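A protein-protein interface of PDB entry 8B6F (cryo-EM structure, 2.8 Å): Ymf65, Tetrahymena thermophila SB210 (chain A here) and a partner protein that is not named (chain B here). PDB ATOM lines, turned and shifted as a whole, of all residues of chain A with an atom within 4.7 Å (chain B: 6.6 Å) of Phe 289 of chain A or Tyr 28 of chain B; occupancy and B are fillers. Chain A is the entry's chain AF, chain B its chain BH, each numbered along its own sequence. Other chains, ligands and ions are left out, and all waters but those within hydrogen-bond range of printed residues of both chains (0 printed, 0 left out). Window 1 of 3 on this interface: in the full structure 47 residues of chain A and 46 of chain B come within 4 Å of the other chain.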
ATOM      1  N   THR A 285       7.213 -22.090  22.325  1.00  0.00           N
ATOM      2  CA  THR A 285       7.047 -21.150  23.427  1.00  0.00           C
ATOM      3  C   THR A 285       8.326 -20.357  23.658  1.00  0.00           C
ATOM      4  O   THR A 285       8.280 -19.142  23.875  1.00  0.00           O
ATOM      5  CB  THR A 285       6.640 -21.894  24.699  1.00  0.00           C
ATOM      6  OG1 THR A 285       5.391 -22.562  24.485  1.00  0.00           O
ATOM      7  CG2 THR A 285       6.489 -20.927  25.867  1.00  0.00           C
ATOM      8  N   THR A 286       9.478 -21.027  23.611  1.00  0.00           N
ATOM      9  CA  THR A 286      10.745 -20.322  23.767  1.00  0.00           C
ATOM     10  C   THR A 286      10.913 -19.257  22.694  1.00  0.00           C
ATOM     11  O   THR A 286      11.181 -18.090  22.997  1.00  0.00           O
ATOM     12  CB  THR A 286      11.898 -21.319  23.692  1.00  0.00           C
ATOM     13  OG1 THR A 286      11.526 -22.529  24.357  1.00  0.00           O
ATOM     14  CG2 THR A 286      13.139 -20.747  24.349  1.00  0.00           C
ATOM     15  N   PHE A 287      10.774 -19.648  21.427  1.00  0.00           N
ATOM     16  CA  PHE A 287      10.927 -18.690  20.339  1.00  0.00           C
ATOM     17  C   PHE A 287       9.955 -17.535  20.505  1.00  0.00           C
ATOM     18  O   PHE A 287      10.338 -16.363  20.422  1.00  0.00           O
ATOM     19  CB  PHE A 287      10.706 -19.384  18.994  1.00  0.00           C
ATOM     20  CG  PHE A 287      11.694 -20.477  18.701  1.00  0.00           C
ATOM     21  CD1 PHE A 287      12.985 -20.427  19.202  1.00  0.00           C
ATOM     22  CD2 PHE A 287      11.324 -21.561  17.925  1.00  0.00           C
ATOM     23  CE1 PHE A 287      13.887 -21.436  18.932  1.00  0.00           C
ATOM     24  CE2 PHE A 287      12.223 -22.574  17.654  1.00  0.00           C
ATOM     25  CZ  PHE A 287      13.505 -22.510  18.157  1.00  0.00           C
ATOM     26  N   TYR A 288       8.682 -17.856  20.730  1.00  0.00           N
ATOM     27  CA  TYR A 288       7.656 -16.832  20.866  1.00  0.00           C
ATOM     28  C   TYR A 288       8.029 -15.824  21.948  1.00  0.00           C
ATOM     29  O   TYR A 288       8.231 -14.637  21.669  1.00  0.00           O
ATOM     30  CB  TYR A 288       6.321 -17.516  21.176  1.00  0.00           C
ATOM     31  CG  TYR A 288       5.249 -16.597  21.693  1.00  0.00           C
ATOM     32  CD1 TYR A 288       4.401 -15.938  20.819  1.00  0.00           C
ATOM     33  CD2 TYR A 288       5.065 -16.412  23.054  1.00  0.00           C
ATOM     34  CE1 TYR A 288       3.412 -15.107  21.283  1.00  0.00           C
ATOM     35  CE2 TYR A 288       4.081 -15.583  23.528  1.00  0.00           C
ATOM     36  CZ  TYR A 288       3.262 -14.928  22.636  1.00  0.00           C
ATOM     37  OH  TYR A 288       2.281 -14.104  23.108  1.00  0.00           O
ATOM     38  N   PHE A 289       8.113 -16.281  23.201  1.00  0.00           N
ATOM     39  CA  PHE A 289       8.322 -15.351  24.308  1.00  0.00           C
ATOM     40  C   PHE A 289       9.648 -14.616  24.192  1.00  0.00           C
ATOM     41  O   PHE A 289       9.719 -13.406  24.432  1.00  0.00           O
ATOM     42  CB  PHE A 289       8.245 -16.084  25.647  1.00  0.00           C
ATOM     43  CG  PHE A 289       6.904 -15.992  26.302  1.00  0.00           C
ATOM     44  CD1 PHE A 289       6.498 -14.811  26.895  1.00  0.00           C
ATOM     45  CD2 PHE A 289       6.051 -17.078  26.327  1.00  0.00           C
ATOM     46  CE1 PHE A 289       5.265 -14.712  27.497  1.00  0.00           C
ATOM     47  CE2 PHE A 289       4.817 -16.984  26.930  1.00  0.00           C
ATOM     48  CZ  PHE A 289       4.423 -15.800  27.516  1.00  0.00           C
ATOM     49  N   LEU A 290      10.714 -15.327  23.828  1.00  0.00           N
ATOM     50  CA  LEU A 290      12.037 -14.725  23.877  1.00  0.00           C
ATOM     51  C   LEU A 290      12.335 -13.817  22.692  1.00  0.00           C
ATOM     52  O   LEU A 290      13.252 -12.995  22.788  1.00  0.00           O
ATOM     53  CB  LEU A 290      13.098 -15.827  23.967  1.00  0.00           C
ATOM     54  CG  LEU A 290      14.528 -15.393  24.299  1.00  0.00           C
ATOM     55  CD1 LEU A 290      14.607 -14.658  25.626  1.00  0.00           C
ATOM     56  CD2 LEU A 290      15.441 -16.605  24.312  1.00  0.00           C
ATOM     57  N   ILE A 291      11.595 -13.932  21.589  1.00  0.00           N
ATOM     58  CA  ILE A 291      11.877 -13.102  20.422  1.00  0.00           C
ATOM     59  C   ILE A 291      10.644 -12.314  20.003  1.00  0.00           C
ATOM     60  O   ILE A 291      10.668 -11.078  19.980  1.00  0.00           O
ATOM     61  CB  ILE A 291      12.407 -13.954  19.254  1.00  0.00           C
ATOM     62  CG1 ILE A 291      13.717 -14.638  19.654  1.00  0.00           C
ATOM     63  CG2 ILE A 291      12.622 -13.097  18.015  1.00  0.00           C
ATOM     64  CD1 ILE A 291      13.535 -16.026  20.214  1.00  0.00           C
ATOM     65  N   PHE A 293       7.482 -11.817  21.274  1.00  0.00           N
ATOM     66  CA  PHE A 293       6.862 -10.938  22.255  1.00  0.00           C
ATOM     67  C   PHE A 293       7.835  -9.876  22.743  1.00  0.00           C
ATOM     68  O   PHE A 293       7.428  -8.742  23.018  1.00  0.00           O
ATOM     69  CB  PHE A 293       6.327 -11.756  23.430  1.00  0.00           C
ATOM     70  CG  PHE A 293       5.395 -10.988  24.317  1.00  0.00           C
ATOM     71  CD1 PHE A 293       4.038 -10.951  24.047  1.00  0.00           C
ATOM     72  CD2 PHE A 293       5.876 -10.289  25.410  1.00  0.00           C
ATOM     73  CE1 PHE A 293       3.179 -10.241  24.855  1.00  0.00           C
ATOM     74  CE2 PHE A 293       5.020  -9.577  26.223  1.00  0.00           C
ATOM     75  CZ  PHE A 293       3.670  -9.553  25.945  1.00  0.00           C
ATOM     76  N   LEU A 294       9.120 -10.220  22.857  1.00  0.00           N
ATOM     77  CA  LEU A 294      10.108  -9.238  23.289  1.00  0.00           C
ATOM     78  C   LEU A 294      10.242  -8.108  22.276  1.00  0.00           C
ATOM     79  O   LEU A 294      10.341  -6.936  22.654  1.00  0.00           O
ATOM     80  CB  LEU A 294      11.457  -9.916  23.526  1.00  0.00           C
ATOM     81  CG  LEU A 294      12.574  -9.031  24.088  1.00  0.00           C
ATOM     82  CD1 LEU A 294      12.129  -8.299  25.345  1.00  0.00           C
ATOM     83  CD2 LEU A 294      13.815  -9.860  24.377  1.00  0.00           C
ATOM     84  N   LEU A 340      -1.721 -25.197  28.410  1.00  0.00           N
ATOM     85  CA  LEU A 340      -0.430 -24.578  28.125  1.00  0.00           C
ATOM     86  C   LEU A 340      -0.605 -23.304  27.310  1.00  0.00           C
ATOM     87  O   LEU A 340       0.026 -22.280  27.593  1.00  0.00           O
ATOM     88  CB  LEU A 340       0.476 -25.564  27.390  1.00  0.00           C
ATOM     89  CG  LEU A 340       0.834 -26.841  28.150  1.00  0.00           C
ATOM     90  CD1 LEU A 340       1.582 -27.794  27.240  1.00  0.00           C
ATOM     91  CD2 LEU A 340       1.658 -26.530  29.388  1.00  0.00           C
ATOM     92  N   SER A 343      -2.020 -20.558  29.497  1.00  0.00           N
ATOM     93  CA  SER A 343      -0.975 -20.035  30.367  1.00  0.00           C
ATOM     94  C   SER A 343      -0.139 -19.004  29.622  1.00  0.00           C
ATOM     95  O   SER A 343       0.148 -17.921  30.145  1.00  0.00           O
ATOM     96  CB  SER A 343      -0.092 -21.174  30.877  1.00  0.00           C
ATOM     97  OG  SER A 343      -0.868 -22.170  31.518  1.00  0.00           O
ATOM     98  N   THR A 344       0.270 -19.330  28.397  1.00  0.00           N
ATOM     99  CA  THR A 344       1.023 -18.378  27.588  1.00  0.00           C
ATOM    100  C   THR A 344       0.221 -17.104  27.355  1.00  0.00           C
ATOM    101  O   THR A 344       0.763 -15.996  27.430  1.00  0.00           O
ATOM    102  CB  THR A 344       1.412 -19.029  26.258  1.00  0.00           C
ATOM    103  OG1 THR A 344       2.464 -19.979  26.475  1.00  0.00           O
ATOM    104  CG2 THR A 344       1.863 -17.994  25.232  1.00  0.00           C
ATOM    105  N   ASN A 347       0.017 -14.913  30.570  1.00  0.00           N
ATOM    106  CA  ASN A 347       1.295 -14.250  30.800  1.00  0.00           C
ATOM    107  C   ASN A 347       1.518 -13.135  29.791  1.00  0.00           C
ATOM    108  O   ASN A 347       2.079 -12.086  30.126  1.00  0.00           O
ATOM    109  CB  ASN A 347       2.432 -15.266  30.749  1.00  0.00           C
ATOM    110  CG  ASN A 347       2.478 -16.142  31.982  1.00  0.00           C
ATOM    111  OD1 ASN A 347       3.191 -15.849  32.940  1.00  0.00           O
ATOM    112  ND2 ASN A 347       1.706 -17.222  31.969  1.00  0.00           N
ATOM    113  N   SER A 348       1.086 -13.344  28.550  1.00  0.00           N
ATOM    114  CA  SER A 348       1.210 -12.298  27.543  1.00  0.00           C
ATOM    115  C   SER A 348       0.405 -11.066  27.926  1.00  0.00           C
ATOM    116  O   SER A 348       0.880  -9.935  27.777  1.00  0.00           O
ATOM    117  CB  SER A 348       0.710 -12.834  26.204  1.00  0.00           C
ATOM    118  OG  SER A 348       1.478 -13.937  25.773  1.00  0.00           O
ATOM    119  N   PHE A 351       2.186  -9.238  30.732  1.00  0.00           N
ATOM    120  CA  PHE A 351       3.336  -8.501  30.234  1.00  0.00           C
ATOM    121  C   PHE A 351       2.909  -7.283  29.426  1.00  0.00           C
ATOM    122  O   PHE A 351       3.613  -6.268  29.423  1.00  0.00           O
ATOM    123  CB  PHE A 351       4.226  -9.426  29.400  1.00  0.00           C
ATOM    124  CG  PHE A 351       4.741 -10.626  30.156  1.00  0.00           C
ATOM    125  CD1 PHE A 351       4.673 -10.687  31.538  1.00  0.00           C
ATOM    126  CD2 PHE A 351       5.302 -11.694  29.476  1.00  0.00           C
ATOM    127  CE1 PHE A 351       5.145 -11.787  32.223  1.00  0.00           C
ATOM    128  CE2 PHE A 351       5.775 -12.798  30.156  1.00  0.00           C
ATOM    129  CZ  PHE A 351       5.697 -12.844  31.531  1.00  0.00           C
ATOM    130  N   LEU B  23      13.050  -9.732  33.249  1.00  0.00           N
ATOM    131  CA  LEU B  23      13.027 -10.654  34.378  1.00  0.00           C
ATOM    132  C   LEU B  23      11.767 -11.508  34.365  1.00  0.00           C
ATOM    133  O   LEU B  23      11.826 -12.719  34.606  1.00  0.00           O
ATOM    134  CB  LEU B  23      13.134  -9.874  35.687  1.00  0.00           C
ATOM    135  CG  LEU B  23      13.158 -10.711  36.965  1.00  0.00           C
ATOM    136  CD1 LEU B  23      14.381 -11.612  36.998  1.00  0.00           C
ATOM    137  CD2 LEU B  23      13.132  -9.803  38.172  1.00  0.00           C
ATOM    138  N   ASN B  24      10.612 -10.895  34.096  1.00  0.00           N
ATOM    139  CA  ASN B  24       9.375 -11.666  34.037  1.00  0.00           C
ATOM    140  C   ASN B  24       9.420 -12.693  32.915  1.00  0.00           C
ATOM    141  O   ASN B  24       9.006 -13.843  33.098  1.00  0.00           O
ATOM    142  CB  ASN B  24       8.181 -10.732  33.856  1.00  0.00           C
ATOM    143  CG  ASN B  24       7.781 -10.045  35.140  1.00  0.00           C
ATOM    144  OD1 ASN B  24       8.604  -9.833  36.027  1.00  0.00           O
ATOM    145  ND2 ASN B  24       6.505  -9.700  35.251  1.00  0.00           N
ATOM    146  N   ILE B  25       9.907 -12.294  31.738  1.00  0.00           N
ATOM    147  CA  ILE B  25       9.991 -13.231  30.620  1.00  0.00           C
ATOM    148  C   ILE B  25      10.910 -14.391  30.974  1.00  0.00           C
ATOM    149  O   ILE B  25      10.596 -15.557  30.705  1.00  0.00           O
ATOM    150  CB  ILE B  25      10.460 -12.498  29.348  1.00  0.00           C
ATOM    151  CG1 ILE B  25       9.374 -11.530  28.871  1.00  0.00           C
ATOM    152  CG2 ILE B  25      10.808 -13.497  28.246  1.00  0.00           C
ATOM    153  CD1 ILE B  25       9.803 -10.634  27.732  1.00  0.00           C
ATOM    154  N   ILE B  26      12.063 -14.092  31.574  1.00  0.00           N
ATOM    155  CA  ILE B  26      13.019 -15.140  31.921  1.00  0.00           C
ATOM    156  C   ILE B  26      12.430 -16.074  32.970  1.00  0.00           C
ATOM    157  O   ILE B  26      12.580 -17.298  32.883  1.00  0.00           O
ATOM    158  CB  ILE B  26      14.347 -14.517  32.392  1.00  0.00           C
ATOM    159  CG1 ILE B  26      15.059 -13.850  31.213  1.00  0.00           C
ATOM    160  CG2 ILE B  26      15.246 -15.572  33.029  1.00  0.00           C
ATOM    161  CD1 ILE B  26      16.274 -13.038  31.601  1.00  0.00           C
ATOM    162  N   ASN B  27      11.752 -15.517  33.975  1.00  0.00           N
ATOM    163  CA  ASN B  27      11.155 -16.362  35.004  1.00  0.00           C
ATOM    164  C   ASN B  27      10.090 -17.277  34.418  1.00  0.00           C
ATOM    165  O   ASN B  27      10.036 -18.466  34.753  1.00  0.00           O
ATOM    166  CB  ASN B  27      10.561 -15.499  36.117  1.00  0.00           C
ATOM    167  CG  ASN B  27      11.617 -14.743  36.896  1.00  0.00           C
ATOM    168  OD1 ASN B  27      12.755 -14.605  36.451  1.00  0.00           O
ATOM    169  ND2 ASN B  27      11.244 -14.253  38.071  1.00  0.00           N
ATOM    170  N   TYR B  28       9.232 -16.751  33.544  1.00  0.00           N
ATOM    171  CA  TYR B  28       8.224 -17.605  32.926  1.00  0.00           C
ATOM    172  C   TYR B  28       8.866 -18.690  32.072  1.00  0.00           C
ATOM    173  O   TYR B  28       8.419 -19.842  32.083  1.00  0.00           O
ATOM    174  CB  TYR B  28       7.260 -16.780  32.079  1.00  0.00           C
ATOM    175  CG  TYR B  28       6.262 -17.654  31.360  1.00  0.00           C
ATOM    176  CD1 TYR B  28       5.135 -18.133  32.012  1.00  0.00           C
ATOM    177  CD2 TYR B  28       6.465 -18.026  30.041  1.00  0.00           C
ATOM    178  CE1 TYR B  28       4.229 -18.945  31.363  1.00  0.00           C
ATOM    179  CE2 TYR B  28       5.566 -18.836  29.384  1.00  0.00           C
ATOM    180  CZ  TYR B  28       4.449 -19.292  30.049  1.00  0.00           C
ATOM    181  OH  TYR B  28       3.550 -20.101  29.396  1.00  0.00           O
ATOM    182  N   LEU B  29       9.911 -18.343  31.317  1.00  0.00           N
ATOM    183  CA  LEU B  29      10.590 -19.346  30.506  1.00  0.00           C
ATOM    184  C   LEU B  29      11.206 -20.429  31.378  1.00  0.00           C
ATOM    185  O   LEU B  29      11.169 -21.614  31.030  1.00  0.00           O
ATOM    186  CB  LEU B  29      11.659 -18.687  29.633  1.00  0.00           C
ATOM    187  CG  LEU B  29      11.188 -17.982  28.356  1.00  0.00           C
ATOM    188  CD1 LEU B  29      12.351 -17.276  27.681  1.00  0.00           C
ATOM    189  CD2 LEU B  29      10.530 -18.953  27.388  1.00  0.00           C
ATOM    190  N   ILE B  30      11.780 -20.043  32.519  1.00  0.00           N
ATOM    191  CA  ILE B  30      12.398 -21.026  33.404  1.00  0.00           C
ATOM    192  C   ILE B  30      11.349 -21.977  33.960  1.00  0.00           C
ATOM    193  O   ILE B  30      11.558 -23.195  34.007  1.00  0.00           O
ATOM    194  CB  ILE B  30      13.171 -20.311  34.526  1.00  0.00           C
ATOM    195  CG1 ILE B  30      14.375 -19.571  33.950  1.00  0.00           C
ATOM    196  CG2 ILE B  30      13.624 -21.296  35.594  1.00  0.00           C
ATOM    197  CD1 ILE B  30      14.853 -18.447  34.823  1.00  0.00           C
ATOM    198  N   VAL B  31      10.212 -21.442  34.409  1.00  0.00           N
ATOM    199  CA  VAL B  31       9.180 -22.303  34.976  1.00  0.00           C
ATOM    200  C   VAL B  31       8.563 -23.176  33.892  1.00  0.00           C
ATOM    201  O   VAL B  31       8.276 -24.358  34.114  1.00  0.00           O
ATOM    202  CB  VAL B  31       8.119 -21.462  35.709  1.00  0.00           C
ATOM    203  CG1 VAL B  31       7.032 -22.358  36.275  1.00  0.00           C
ATOM    204  CG2 VAL B  31       8.761 -20.654  36.821  1.00  0.00           C
ATOM    205  N   PHE B  32       8.349 -22.611  32.701  1.00  0.00           N
ATOM    206  CA  PHE B  32       7.848 -23.405  31.586  1.00  0.00           C
ATOM    207  C   PHE B  32       8.819 -24.523  31.242  1.00  0.00           C
ATOM    208  O   PHE B  32       8.408 -25.654  30.959  1.00  0.00           O
ATOM    209  CB  PHE B  32       7.606 -22.514  30.369  1.00  0.00           C
ATOM    210  CG  PHE B  32       7.174 -23.269  29.146  1.00  0.00           C
ATOM    211  CD1 PHE B  32       5.836 -23.538  28.918  1.00  0.00           C
ATOM    212  CD2 PHE B  32       8.109 -23.707  28.222  1.00  0.00           C
ATOM    213  CE1 PHE B  32       5.436 -24.232  27.792  1.00  0.00           C
ATOM    214  CE2 PHE B  32       7.716 -24.399  27.096  1.00  0.00           C
ATOM    215  CZ  PHE B  32       6.377 -24.662  26.880  1.00  0.00           C
ATOM    216  N   MET B  33      10.114 -24.220  31.259  1.00  0.00           N
ATOM    217  CA  MET B  33      11.126 -25.236  31.004  1.00  0.00           C
ATOM    218  C   MET B  33      11.084 -26.330  32.062  1.00  0.00           C
ATOM    219  O   MET B  33      11.229 -27.516  31.745  1.00  0.00           O
ATOM    220  CB  MET B  33      12.501 -24.577  30.958  1.00  0.00           C
ATOM    221  CG  MET B  33      13.654 -25.511  30.663  1.00  0.00           C
ATOM    222  SD  MET B  33      15.164 -24.909  31.430  1.00  0.00           S
ATOM    223  CE  MET B  33      15.171 -23.199  30.893  1.00  0.00           C
ATOM    224  N   MET B  73       3.958 -21.234  38.752  1.00  0.00           N
ATOM    225  CA  MET B  73       3.228 -20.583  37.669  1.00  0.00           C
ATOM    226  C   MET B  73       2.060 -19.774  38.213  1.00  0.00           C
ATOM    227  O   MET B  73       1.775 -18.674  37.727  1.00  0.00           O
ATOM    228  CB  MET B  73       2.733 -21.622  36.663  1.00  0.00           C
ATOM    229  CG  MET B  73       3.845 -22.349  35.928  1.00  0.00           C
ATOM    230  SD  MET B  73       3.239 -23.517  34.694  1.00  0.00           S
ATOM    231  CE  MET B  73       2.676 -22.397  33.417  1.00  0.00           C
ATOM    232  N   LEU B  80       9.241 -18.890  42.238  1.00  0.00           N
ATOM    233  CA  LEU B  80       9.923 -17.979  41.323  1.00  0.00           C
ATOM    234  C   LEU B  80       8.955 -16.995  40.678  1.00  0.00           C
ATOM    235  O   LEU B  80       9.254 -15.799  40.581  1.00  0.00           O
ATOM    236  CB  LEU B  80      10.664 -18.777  40.250  1.00  0.00           C
ATOM    237  CG  LEU B  80      11.675 -17.999  39.402  1.00  0.00           C
ATOM    238  CD1 LEU B  80      12.835 -17.499  40.246  1.00  0.00           C
ATOM    239  CD2 LEU B  80      12.183 -18.855  38.254  1.00  0.00           C
ATOM    240  N   GLY B  81       7.801 -17.475  40.215  1.00  0.00           N
ATOM    241  CA  GLY B  81       6.863 -16.590  39.546  1.00  0.00           C
ATOM    242  C   GLY B  81       6.411 -15.437  40.419  1.00  0.00           C
ATOM    243  O   GLY B  81       6.058 -14.371  39.910  1.00  0.00           O
ATOM    244  N   TYR B 115      -4.481 -22.110  37.453  1.00  0.00           N
ATOM    245  CA  TYR B 115      -3.386 -23.054  37.655  1.00  0.00           C
ATOM    246  C   TYR B 115      -3.676 -24.001  38.813  1.00  0.00           C
ATOM    247  O   TYR B 115      -3.366 -25.194  38.742  1.00  0.00           O
ATOM    248  CB  TYR B 115      -2.081 -22.300  37.913  1.00  0.00           C
ATOM    249  CG  TYR B 115      -1.571 -21.538  36.718  1.00  0.00           C
ATOM    250  CD1 TYR B 115      -1.108 -22.204  35.594  1.00  0.00           C
ATOM    251  CD2 TYR B 115      -1.531 -20.153  36.721  1.00  0.00           C
ATOM    252  CE1 TYR B 115      -0.636 -21.512  34.500  1.00  0.00           C
ATOM    253  CE2 TYR B 115      -1.062 -19.451  35.633  1.00  0.00           C
ATOM    254  CZ  TYR B 115      -0.616 -20.136  34.525  1.00  0.00           C
ATOM    255  OH  TYR B 115      -0.144 -19.439  33.439  1.00  0.00           O
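Printed residues of chain B that touch a printed residue of chain A: Asn 24, Ile 25, Tyr 28, Leu 29, Phe 32, Met 73 and Tyr 115. Hydrophobic or aromatic side chains of chain B that line the printed part of chain A: Ile 25, Tyr 28, Leu 29, Phe 32, Met 73 and Tyr 115. Printed residues of chain A that touch a printed residue of chain B: Thr 285, Thr 286, Phe 289, Ser 343, Thr 344, Asn 347 and Phe 351. Hydrophobic or aromatic side chains of chain A that line the printed part of chain B: Phe 289 and Phe 351.
OH of Tyr 115 of chain B lies close to OG of Ser 343 of chain A, 3.4 Å away. OH of Tyr 28 of chain B lies within hydrogen-bond range of OG1 of Thr 344 of chain A. OH of Tyr 115 of chain B sits at hydrogen-bond distance from ND2 of Asn 347 of chain A, 3.2 Å away.
Among the printed residues, pairs that only touch across the chains: Thr 285 of chain A with Phe 32 of chain B (3.3 Å), Thr 286 of chain A with Leu 29 of chain B (3.9 Å), Phe 289 of chain A with Ile 25 of chain B (3.97 Å), Phe 289 of chain A with Tyr 28 of chain B (3.2 Å), Ser 343 of chain A with Tyr 28 of chain B (3.9 Å), Ser 343 of chain A with Met 73 of chain B (3.95 Å), Asn 347 of chain A with Tyr 28 of chain B (3.1 Å) and Phe 351 of chain A with Asn 24 of chain B (3.6 Å).
The backbone carbonyl oxygen of Ser 343 of chain A lies within hydrogen-bond range of the side-chain amide nitrogen of Asn 347 of chain A, 2.5 Å away. The backbone carbonyl oxygen (O) of Thr 344 of chain A sits at hydrogen-bond distance from the side-chain hydroxyl (OG) of Ser 348 of chain A.
Of the printed residues of chain B, Phe 289 of chain A touches Ile 25 (3.97 Å) and Tyr 28 (3.2 Å). Of the printed residues of chain B, Thr 286 of chain A touches Leu 29 (3.9 Å). Printed residues of chain B within 4 Å of Asn 347 of chain A: Tyr 28 and Tyr 115. Ile 26 of chain B touches none of the printed residues of chain A. Leu 340 of chain A touches none of the printed residues of chain B. The nearest residue of chain A that does not touch Tyr 28 of chain B is Thr 285 of chain A (4.2 Å).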
